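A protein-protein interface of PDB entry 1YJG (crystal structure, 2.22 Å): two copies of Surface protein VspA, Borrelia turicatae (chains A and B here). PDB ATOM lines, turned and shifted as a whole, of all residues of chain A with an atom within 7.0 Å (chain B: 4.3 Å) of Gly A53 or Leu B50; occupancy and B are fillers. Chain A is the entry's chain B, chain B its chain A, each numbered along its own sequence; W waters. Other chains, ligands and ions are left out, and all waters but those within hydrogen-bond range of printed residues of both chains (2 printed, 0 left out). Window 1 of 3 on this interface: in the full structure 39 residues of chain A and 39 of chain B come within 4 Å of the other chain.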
ATOM      1  N   ILE A  24     -12.716 -13.106  -6.905  1.00  0.00           N
ATOM      2  CA  ILE A  24     -13.914 -13.234  -6.095  1.00  0.00           C
ATOM      3  C   ILE A  24     -13.614 -14.162  -4.904  1.00  0.00           C
ATOM      4  O   ILE A  24     -14.194 -13.987  -3.829  1.00  0.00           O
ATOM      5  CB  ILE A  24     -15.131 -13.724  -6.913  1.00  0.00           C
ATOM      6  CG1 ILE A  24     -15.384 -12.833  -8.136  1.00  0.00           C
ATOM      7  CG2 ILE A  24     -16.381 -13.726  -6.038  1.00  0.00           C
ATOM      8  CD1 ILE A  24     -15.509 -11.328  -7.833  1.00  0.00           C
ATOM      9  N   LEU A  27     -12.286 -12.086  -2.228  1.00  0.00           N
ATOM     10  CA  LEU A  27     -13.336 -11.291  -1.605  1.00  0.00           C
ATOM     11  C   LEU A  27     -14.121 -12.179  -0.630  1.00  0.00           C
ATOM     12  O   LEU A  27     -14.596 -11.708   0.402  1.00  0.00           O
ATOM     13  CB  LEU A  27     -14.294 -10.740  -2.657  1.00  0.00           C
ATOM     14  CG  LEU A  27     -13.714  -9.746  -3.656  1.00  0.00           C
ATOM     15  CD1 LEU A  27     -14.764  -9.384  -4.719  1.00  0.00           C
ATOM     16  CD2 LEU A  27     -13.196  -8.512  -2.931  1.00  0.00           C
ATOM     17  N   ALA A  30     -13.002 -12.318   2.989  1.00  0.00           N
ATOM     18  CA  ALA A  30     -13.324 -11.155   3.811  1.00  0.00           C
ATOM     19  C   ALA A  30     -14.745 -11.166   4.377  1.00  0.00           C
ATOM     20  O   ALA A  30     -15.145 -10.220   5.067  1.00  0.00           O
ATOM     21  CB  ALA A  30     -13.118  -9.883   3.001  1.00  0.00           C
ATOM     22  N   LYS A  33     -15.619 -10.341   8.168  1.00  0.00           N
ATOM     23  CA  LYS A  33     -14.298  -9.912   8.618  1.00  0.00           C
ATOM     24  C   LYS A  33     -14.124  -8.404   8.479  1.00  0.00           C
ATOM     25  O   LYS A  33     -14.590  -7.791   7.523  1.00  0.00           O
ATOM     26  CB  LYS A  33     -13.188 -10.579   7.797  1.00  0.00           C
ATOM     27  CG  LYS A  33     -13.128 -12.095   7.836  1.00  0.00           C
ATOM     28  CD  LYS A  33     -12.299 -12.600   9.015  1.00  0.00           C
ATOM     29  CE  LYS A  33     -12.467 -14.098   9.203  1.00  0.00           C
ATOM     30  NZ  LYS A  33     -12.171 -14.840   7.945  1.00  0.00           N
ATOM     31  N   ILE A  35     -11.198  -5.049   9.120  1.00  0.00           N
ATOM     32  CA  ILE A  35      -9.775  -4.792   9.090  1.00  0.00           C
ATOM     33  C   ILE A  35      -9.430  -4.441  10.527  1.00  0.00           C
ATOM     34  O   ILE A  35      -9.851  -3.401  11.039  1.00  0.00           O
ATOM     35  CB  ILE A  35      -9.427  -3.634   8.142  1.00  0.00           C
ATOM     36  CG1 ILE A  35      -9.795  -4.020   6.708  1.00  0.00           C
ATOM     37  CG2 ILE A  35      -7.936  -3.285   8.238  1.00  0.00           C
ATOM     38  CD1 ILE A  35      -9.679  -2.891   5.730  1.00  0.00           C
ATOM     39  N   LYS A  46     -23.297  -8.014   7.936  1.00  0.00           N
ATOM     40  CA  LYS A  46     -23.192  -6.688   7.314  1.00  0.00           C
ATOM     41  C   LYS A  46     -22.354  -6.758   6.024  1.00  0.00           C
ATOM     42  O   LYS A  46     -21.590  -5.846   5.716  1.00  0.00           O
ATOM     43  CB  LYS A  46     -22.586  -5.677   8.297  1.00  0.00           C
ATOM     44  CG  LYS A  46     -23.185  -5.697   9.714  1.00  0.00           C
ATOM     45  CD  LYS A  46     -22.131  -5.356  10.770  1.00  0.00           C
ATOM     46  CE  LYS A  46     -22.603  -5.676  12.185  1.00  0.00           C
ATOM     47  NZ  LYS A  46     -23.756  -4.829  12.620  1.00  0.00           N
ATOM     48  N   ASN A  47     -22.550  -7.823   5.254  1.00  0.00           N
ATOM     49  CA  ASN A  47     -21.795  -8.055   4.022  1.00  0.00           C
ATOM     50  C   ASN A  47     -22.281  -7.423   2.712  1.00  0.00           C
ATOM     51  O   ASN A  47     -21.604  -7.556   1.686  1.00  0.00           O
ATOM     52  CB  ASN A  47     -21.661  -9.568   3.822  1.00  0.00           C
ATOM     53  CG  ASN A  47     -20.843 -10.225   4.912  1.00  0.00           C
ATOM     54  OD1 ASN A  47     -19.618 -10.106   4.932  1.00  0.00           O
ATOM     55  ND2 ASN A  47     -21.509 -10.913   5.829  1.00  0.00           N
ATOM     56  N   ALA A  48     -23.413  -6.726   2.737  1.00  0.00           N
ATOM     57  CA  ALA A  48     -23.968  -6.107   1.524  1.00  0.00           C
ATOM     58  C   ALA A  48     -22.946  -5.459   0.588  1.00  0.00           C
ATOM     59  O   ALA A  48     -22.844  -5.835  -0.570  1.00  0.00           O
ATOM     60  CB  ALA A  48     -25.037  -5.099   1.882  1.00  0.00           C
ATOM     61  N   LYS A  49     -22.183  -4.506   1.112  1.00  0.00           N
ATOM     62  CA  LYS A  49     -21.187  -3.784   0.323  1.00  0.00           C
ATOM     63  C   LYS A  49     -20.086  -4.667  -0.287  1.00  0.00           C
ATOM     64  O   LYS A  49     -19.589  -4.366  -1.363  1.00  0.00           O
ATOM     65  CB  LYS A  49     -20.620  -2.607   1.127  1.00  0.00           C
ATOM     66  CG  LYS A  49     -21.319  -1.284   0.841  1.00  0.00           C
ATOM     67  CD  LYS A  49     -22.795  -1.307   1.218  1.00  0.00           C
ATOM     68  CE  LYS A  49     -23.526  -0.064   0.715  1.00  0.00           C
ATOM     69  NZ  LYS A  49     -24.396   0.531   1.757  1.00  0.00           N
ATOM     70  N   LEU A  50     -19.709  -5.738   0.398  1.00  0.00           N
ATOM     71  CA  LEU A  50     -18.696  -6.655  -0.104  1.00  0.00           C
ATOM     72  C   LEU A  50     -19.261  -7.393  -1.323  1.00  0.00           C
ATOM     73  O   LEU A  50     -18.558  -7.575  -2.325  1.00  0.00           O
ATOM     74  CB  LEU A  50     -18.272  -7.654   0.977  1.00  0.00           C
ATOM     75  CG  LEU A  50     -17.426  -8.854   0.528  1.00  0.00           C
ATOM     76  CD1 LEU A  50     -16.151  -8.397  -0.144  1.00  0.00           C
ATOM     77  CD2 LEU A  50     -17.103  -9.754   1.708  1.00  0.00           C
ATOM     78  N   ILE A  51     -20.529  -7.807  -1.242  1.00  0.00           N
ATOM     79  CA  ILE A  51     -21.168  -8.508  -2.353  1.00  0.00           C
ATOM     80  C   ILE A  51     -21.319  -7.544  -3.528  1.00  0.00           C
ATOM     81  O   ILE A  51     -21.193  -7.951  -4.681  1.00  0.00           O
ATOM     82  CB  ILE A  51     -22.534  -9.133  -1.983  1.00  0.00           C
ATOM     83  CG1 ILE A  51     -22.497  -9.861  -0.630  1.00  0.00           C
ATOM     84  CG2 ILE A  51     -22.937 -10.133  -3.061  1.00  0.00           C
ATOM     85  CD1 ILE A  51     -21.335 -10.817  -0.453  1.00  0.00           C
ATOM     86  N   SER A  52     -21.588  -6.273  -3.238  1.00  0.00           N
ATOM     87  CA  SER A  52     -21.715  -5.267  -4.277  1.00  0.00           C
ATOM     88  C   SER A  52     -20.374  -5.146  -4.992  1.00  0.00           C
ATOM     89  O   SER A  52     -20.323  -4.886  -6.192  1.00  0.00           O
ATOM     90  CB  SER A  52     -22.081  -3.910  -3.677  1.00  0.00           C
ATOM     91  OG  SER A  52     -23.381  -3.942  -3.135  1.00  0.00           O
ATOM     92  N   GLY A  53     -19.291  -5.305  -4.229  1.00  0.00           N
ATOM     93  CA  GLY A  53     -17.934  -5.232  -4.758  1.00  0.00           C
ATOM     94  C   GLY A  53     -17.705  -6.362  -5.741  1.00  0.00           C
ATOM     95  O   GLY A  53     -17.185  -6.148  -6.822  1.00  0.00           O
ATOM     96  N   ALA A  54     -18.138  -7.556  -5.356  1.00  0.00           N
ATOM     97  CA  ALA A  54     -18.025  -8.753  -6.166  1.00  0.00           C
ATOM     98  C   ALA A  54     -18.894  -8.599  -7.430  1.00  0.00           C
ATOM     99  O   ALA A  54     -18.504  -9.038  -8.517  1.00  0.00           O
ATOM    100  CB  ALA A  54     -18.457  -9.959  -5.354  1.00  0.00           C
ATOM    101  N   TYR A  55     -20.042  -7.929  -7.286  1.00  0.00           N
ATOM    102  CA  TYR A  55     -20.957  -7.696  -8.409  1.00  0.00           C
ATOM    103  C   TYR A  55     -20.263  -6.799  -9.438  1.00  0.00           C
ATOM    104  O   TYR A  55     -20.264  -7.084 -10.638  1.00  0.00           O
ATOM    105  CB  TYR A  55     -22.269  -7.060  -7.934  1.00  0.00           C
ATOM    106  CG  TYR A  55     -23.286  -6.885  -9.045  1.00  0.00           C
ATOM    107  CD1 TYR A  55     -24.250  -7.855  -9.292  1.00  0.00           C
ATOM    108  CD2 TYR A  55     -23.270  -5.754  -9.859  1.00  0.00           C
ATOM    109  CE1 TYR A  55     -25.173  -7.703 -10.316  1.00  0.00           C
ATOM    110  CE2 TYR A  55     -24.183  -5.595 -10.882  1.00  0.00           C
ATOM    111  CZ  TYR A  55     -25.131  -6.571 -11.106  1.00  0.00           C
ATOM    112  OH  TYR A  55     -26.032  -6.424 -12.126  1.00  0.00           O
ATOM    113  N   SER A  56     -19.639  -5.737  -8.950  1.00  0.00           N
ATOM    114  CA  SER A  56     -18.917  -4.789  -9.789  1.00  0.00           C
ATOM    115  C   SER A  56     -17.807  -5.488 -10.586  1.00  0.00           C
ATOM    116  O   SER A  56     -17.638  -5.226 -11.767  1.00  0.00           O
ATOM    117  CB  SER A  56     -18.316  -3.687  -8.918  1.00  0.00           C
ATOM    118  OG  SER A  56     -17.625  -2.736  -9.686  1.00  0.00           O
ATOM    119  N   VAL A  57     -17.085  -6.400  -9.941  1.00  0.00           N
ATOM    120  CA  VAL A  57     -15.999  -7.126 -10.595  1.00  0.00           C
ATOM    121  C   VAL A  57     -16.523  -8.052 -11.701  1.00  0.00           C
ATOM    122  O   VAL A  57     -15.945  -8.123 -12.798  1.00  0.00           O
ATOM    123  CB  VAL A  57     -15.171  -7.944  -9.565  1.00  0.00           C
ATOM    124  CG1 VAL A  57     -14.161  -8.843 -10.259  1.00  0.00           C
ATOM    125  CG2 VAL A  57     -14.460  -7.016  -8.564  1.00  0.00           C
ATOM    126  N   ILE A  58     -17.613  -8.762 -11.422  1.00  0.00           N
ATOM    127  CA  ILE A  58     -18.178  -9.664 -12.414  1.00  0.00           C
ATOM    128  C   ILE A  58     -18.834  -8.866 -13.534  1.00  0.00           C
ATOM    129  O   ILE A  58     -18.955  -9.348 -14.662  1.00  0.00           O
ATOM    130  CB  ILE A  58     -19.121 -10.706 -11.776  1.00  0.00           C
ATOM    131  CG1 ILE A  58     -18.344 -11.561 -10.770  1.00  0.00           C
ATOM    132  CG2 ILE A  58     -19.725 -11.607 -12.847  1.00  0.00           C
ATOM    133  CD1 ILE A  58     -17.053 -12.154 -11.303  1.00  0.00           C
ATOM    134  N   SER A  59     -19.221  -7.635 -13.228  1.00  0.00           N
ATOM    135  CA  SER A  59     -19.826  -6.762 -14.215  1.00  0.00           C
ATOM    136  C   SER A  59     -18.708  -6.368 -15.188  1.00  0.00           C
ATOM    137  O   SER A  59     -18.940  -6.233 -16.391  1.00  0.00           O
ATOM    138  CB  SER A  59     -20.461  -5.538 -13.544  1.00  0.00           C
ATOM    139  OG  SER A  59     -20.777  -4.543 -14.496  1.00  0.00           O
ATOM    140  N   LEU B  27     -13.889  -2.234  -7.222  1.00  0.00           N
ATOM    141  CA  LEU B  27     -14.456  -2.322  -5.879  1.00  0.00           C
ATOM    142  C   LEU B  27     -14.860  -0.936  -5.396  1.00  0.00           C
ATOM    143  O   LEU B  27     -15.841  -0.788  -4.643  1.00  0.00           O
ATOM    144  CB  LEU B  27     -13.446  -2.925  -4.897  1.00  0.00           C
ATOM    145  CG  LEU B  27     -13.003  -4.367  -5.148  1.00  0.00           C
ATOM    146  CD1 LEU B  27     -12.013  -4.786  -4.076  1.00  0.00           C
ATOM    147  CD2 LEU B  27     -14.188  -5.343  -5.194  1.00  0.00           C
ATOM    148  N   ALA B  30     -18.260   0.275  -6.135  1.00  0.00           N
ATOM    149  CA  ALA B  30     -19.304  -0.328  -5.298  1.00  0.00           C
ATOM    150  C   ALA B  30     -19.493   0.383  -3.960  1.00  0.00           C
ATOM    151  O   ALA B  30     -20.369   0.008  -3.180  1.00  0.00           O
ATOM    152  CB  ALA B  30     -18.998  -1.783  -5.050  1.00  0.00           C
ATOM    153  N   ILE B  31     -18.646   1.369  -3.676  1.00  0.00           N
ATOM    154  CA  ILE B  31     -18.747   2.114  -2.432  1.00  0.00           C
ATOM    155  C   ILE B  31     -20.098   2.831  -2.392  1.00  0.00           C
ATOM    156  O   ILE B  31     -20.481   3.515  -3.344  1.00  0.00           O
ATOM    157  CB  ILE B  31     -17.595   3.140  -2.314  1.00  0.00           C
ATOM    158  CG1 ILE B  31     -16.254   2.425  -2.107  1.00  0.00           C
ATOM    159  CG2 ILE B  31     -17.863   4.139  -1.171  1.00  0.00           C
ATOM    160  CD1 ILE B  31     -15.035   3.364  -2.142  1.00  0.00           C
ATOM    161  N   ASN B  47     -19.612   0.647   4.513  1.00  0.00           N
ATOM    162  CA  ASN B  47     -18.608   0.089   3.598  1.00  0.00           C
ATOM    163  C   ASN B  47     -17.494  -0.778   4.182  1.00  0.00           C
ATOM    164  O   ASN B  47     -16.694  -1.318   3.423  1.00  0.00           O
ATOM    165  CB  ASN B  47     -17.954   1.237   2.819  1.00  0.00           C
ATOM    166  CG  ASN B  47     -18.932   1.979   1.953  1.00  0.00           C
ATOM    167  OD1 ASN B  47     -19.402   1.448   0.953  1.00  0.00           O
ATOM    168  ND2 ASN B  47     -19.248   3.212   2.328  1.00  0.00           N
ATOM    169  N   ALA B  48     -17.431  -0.937   5.501  1.00  0.00           N
ATOM    170  CA  ALA B  48     -16.365  -1.747   6.115  1.00  0.00           C
ATOM    171  C   ALA B  48     -15.997  -3.067   5.411  1.00  0.00           C
ATOM    172  O   ALA B  48     -14.828  -3.291   5.102  1.00  0.00           O
ATOM    173  CB  ALA B  48     -16.678  -2.024   7.576  1.00  0.00           C
ATOM    174  N   LYS B  49     -16.984  -3.930   5.170  1.00  0.00           N
ATOM    175  CA  LYS B  49     -16.739  -5.239   4.531  1.00  0.00           C
ATOM    176  C   LYS B  49     -16.179  -5.168   3.115  1.00  0.00           C
ATOM    177  O   LYS B  49     -15.514  -6.102   2.670  1.00  0.00           O
ATOM    178  CB  LYS B  49     -17.993  -6.123   4.575  1.00  0.00           C
ATOM    179  CG  LYS B  49     -17.975  -7.163   5.700  1.00  0.00           C
ATOM    180  CD  LYS B  49     -17.835  -6.497   7.062  1.00  0.00           C
ATOM    181  CE  LYS B  49     -18.060  -7.457   8.217  1.00  0.00           C
ATOM    182  NZ  LYS B  49     -18.860  -6.785   9.286  1.00  0.00           N
ATOM    183  N   LEU B  50     -16.495  -4.089   2.402  1.00  0.00           N
ATOM    184  CA  LEU B  50     -15.997  -3.891   1.046  1.00  0.00           C
ATOM    185  C   LEU B  50     -14.501  -3.559   1.170  1.00  0.00           C
ATOM    186  O   LEU B  50     -13.688  -4.051   0.383  1.00  0.00           O
ATOM    187  CB  LEU B  50     -16.767  -2.775   0.327  1.00  0.00           C
ATOM    188  CG  LEU B  50     -16.235  -2.318  -1.031  1.00  0.00           C
ATOM    189  CD1 LEU B  50     -16.228  -3.474  -2.041  1.00  0.00           C
ATOM    190  CD2 LEU B  50     -17.034  -1.128  -1.551  1.00  0.00           C
ATOM    191  N   ILE B  51     -14.139  -2.748   2.169  1.00  0.00           N
ATOM    192  CA  ILE B  51     -12.737  -2.407   2.376  1.00  0.00           C
ATOM    193  C   ILE B  51     -11.999  -3.689   2.795  1.00  0.00           C
ATOM    194  O   ILE B  51     -10.841  -3.873   2.439  1.00  0.00           O
ATOM    195  CB  ILE B  51     -12.521  -1.305   3.427  1.00  0.00           C
ATOM    196  CG1 ILE B  51     -13.485  -0.129   3.235  1.00  0.00           C
ATOM    197  CG2 ILE B  51     -11.063  -0.796   3.382  1.00  0.00           C
ATOM    198  CD1 ILE B  51     -13.577   0.409   1.821  1.00  0.00           C
ATOM    199  N   SER B  52     -12.664  -4.565   3.549  1.00  0.00           N
ATOM    200  CA  SER B  52     -12.039  -5.817   3.976  1.00  0.00           C
ATOM    201  C   SER B  52     -11.700  -6.628   2.720  1.00  0.00           C
ATOM    202  O   SER B  52     -10.640  -7.239   2.655  1.00  0.00           O
ATOM    203  CB  SER B  52     -12.944  -6.622   4.926  1.00  0.00           C
ATOM    204  OG  SER B  52     -13.179  -5.929   6.153  1.00  0.00           O
ATOM    205  N   GLY B  53     -12.603  -6.615   1.734  1.00  0.00           N
ATOM    206  CA  GLY B  53     -12.418  -7.328   0.480  1.00  0.00           C
ATOM    207  C   GLY B  53     -11.190  -6.829  -0.263  1.00  0.00           C
ATOM    208  O   GLY B  53     -10.380  -7.618  -0.748  1.00  0.00           O
ATOM    209  N   ALA B  54     -11.066  -5.510  -0.349  1.00  0.00           N
ATOM    210  CA  ALA B  54      -9.936  -4.853  -1.003  1.00  0.00           C
ATOM    211  C   ALA B  54      -8.664  -5.241  -0.269  1.00  0.00           C
ATOM    212  O   ALA B  54      -7.654  -5.562  -0.884  1.00  0.00           O
ATOM    213  CB  ALA B  54     -10.105  -3.350  -0.963  1.00  0.00           C
HETATM  214  O   HOH W   1     -19.949  -3.310   5.610  1.00  0.00           O
HETATM  215  O   HOH W   2     -13.085  -3.202   7.591  1.00  0.00           O
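Of the printed residues of chain B, Gly A53 touches Leu B27 (3.5 Å), Ala B30 (3.6 Å) and Leu B50 (3.7 Å). Leu B50 touches two residues of chain A. Of the printed residues of chain A, Asn B47 touches Lys A49. Of the printed residues of chain B, Leu A50 touches Lys B49 and Gly B53. Printed residues of chain A within 4 Å of Ala B30: Ser A52 and Gly A53. Printed residues of chain B within 4 Å of Ile A35: Ile B51 (3.4 Å) and Ser B52 (3.7 Å). The nearest residue of chain A that does not touch Leu B50 is Leu A50 (4.03 Å). The nearest printed residue of chain B that does not touch Ile A35 is Ala B48 (5.2 Å).
The side-chain hydroxyl of Ser B52 is in hydrogen-bond range of the backbone carbonyl oxygen of Ala B48. The backbone carbonyl oxygen (O) of Ala A48 sits at hydrogen-bond distance from the side-chain hydroxyl (OG) of Ser A52 (3.2 Å).
Leu A27 touches Gly B53, and with the chains exchanged Gly A53 touches Leu B27. Ala A30 touches Ser B52, and with the chains exchanged Ser A52 touches Ala B30. Ala A30 touches Gly B53, and with the chains exchanged Gly A53 touches Ala B30. Asn A47 touches Lys B49, and with the chains exchanged Lys A49 touches Asn B47. Of the 18 pairs that touch across the chains among the printed residues, 12 have their exchanged pair printed and touching as well.
Water W1 lies within hydrogen-bond range of O of Lys A46, N of Lys B49 and N of Ala B48. Water W2 lies within hydrogen-bond range of O of Ala B48 (3.0 Å), N of Ile A35 (3.1 Å) and OG of Ser B52 (3.1 Å).
CD2 of Leu A27 touches O of Gly B53 (3.7 Å). Ala A30 touches Ser B52 (CB to C, 3.6 Å). Ala A30 touches Gly B53 (CB to N, 3.5 Å). Ile B51 touches Ile A35. Lys A46 touches Lys B49. OD1 of Asn A47 touches CG of Lys B49, 3.5 Å away. Leu B50 touches Lys A49. Leu B27 touches Gly A53. Gly A53 touches Leu B50. Leu B27 touches Val A57.
The side-chain hydroxyl (OG) of Ser B52 is in hydrogen-bond range of the backbone carbonyl oxygen (O) of Lys A33, at 2.7 Å.
Of the 11 printed residues of chain B, 8 touch a printed residue of chain A. Printed residues of chain A that touch a printed residue of chain B: Leu A27, Ala A30, Lys A33, Ile A35, Lys A46, Asn A47, Lys A49, Leu A50, Ser A52, Gly A53 and Val A57. Hydrophobic or aromatic side chains of chain A within 4 Å of the printed part of chain B: Leu A27, Ala A30, Ile A35, Leu A50 and Val A57. Along chain A the printed residues that touch a printed residue of chain B span positions 27 to 57. Among the printed residues, 18 pairs touch across the chains. Among the printed residues, no Asp or Glu carboxylate lies within 4 Å of a Lys or Arg side-chain nitrogen of the other chain.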
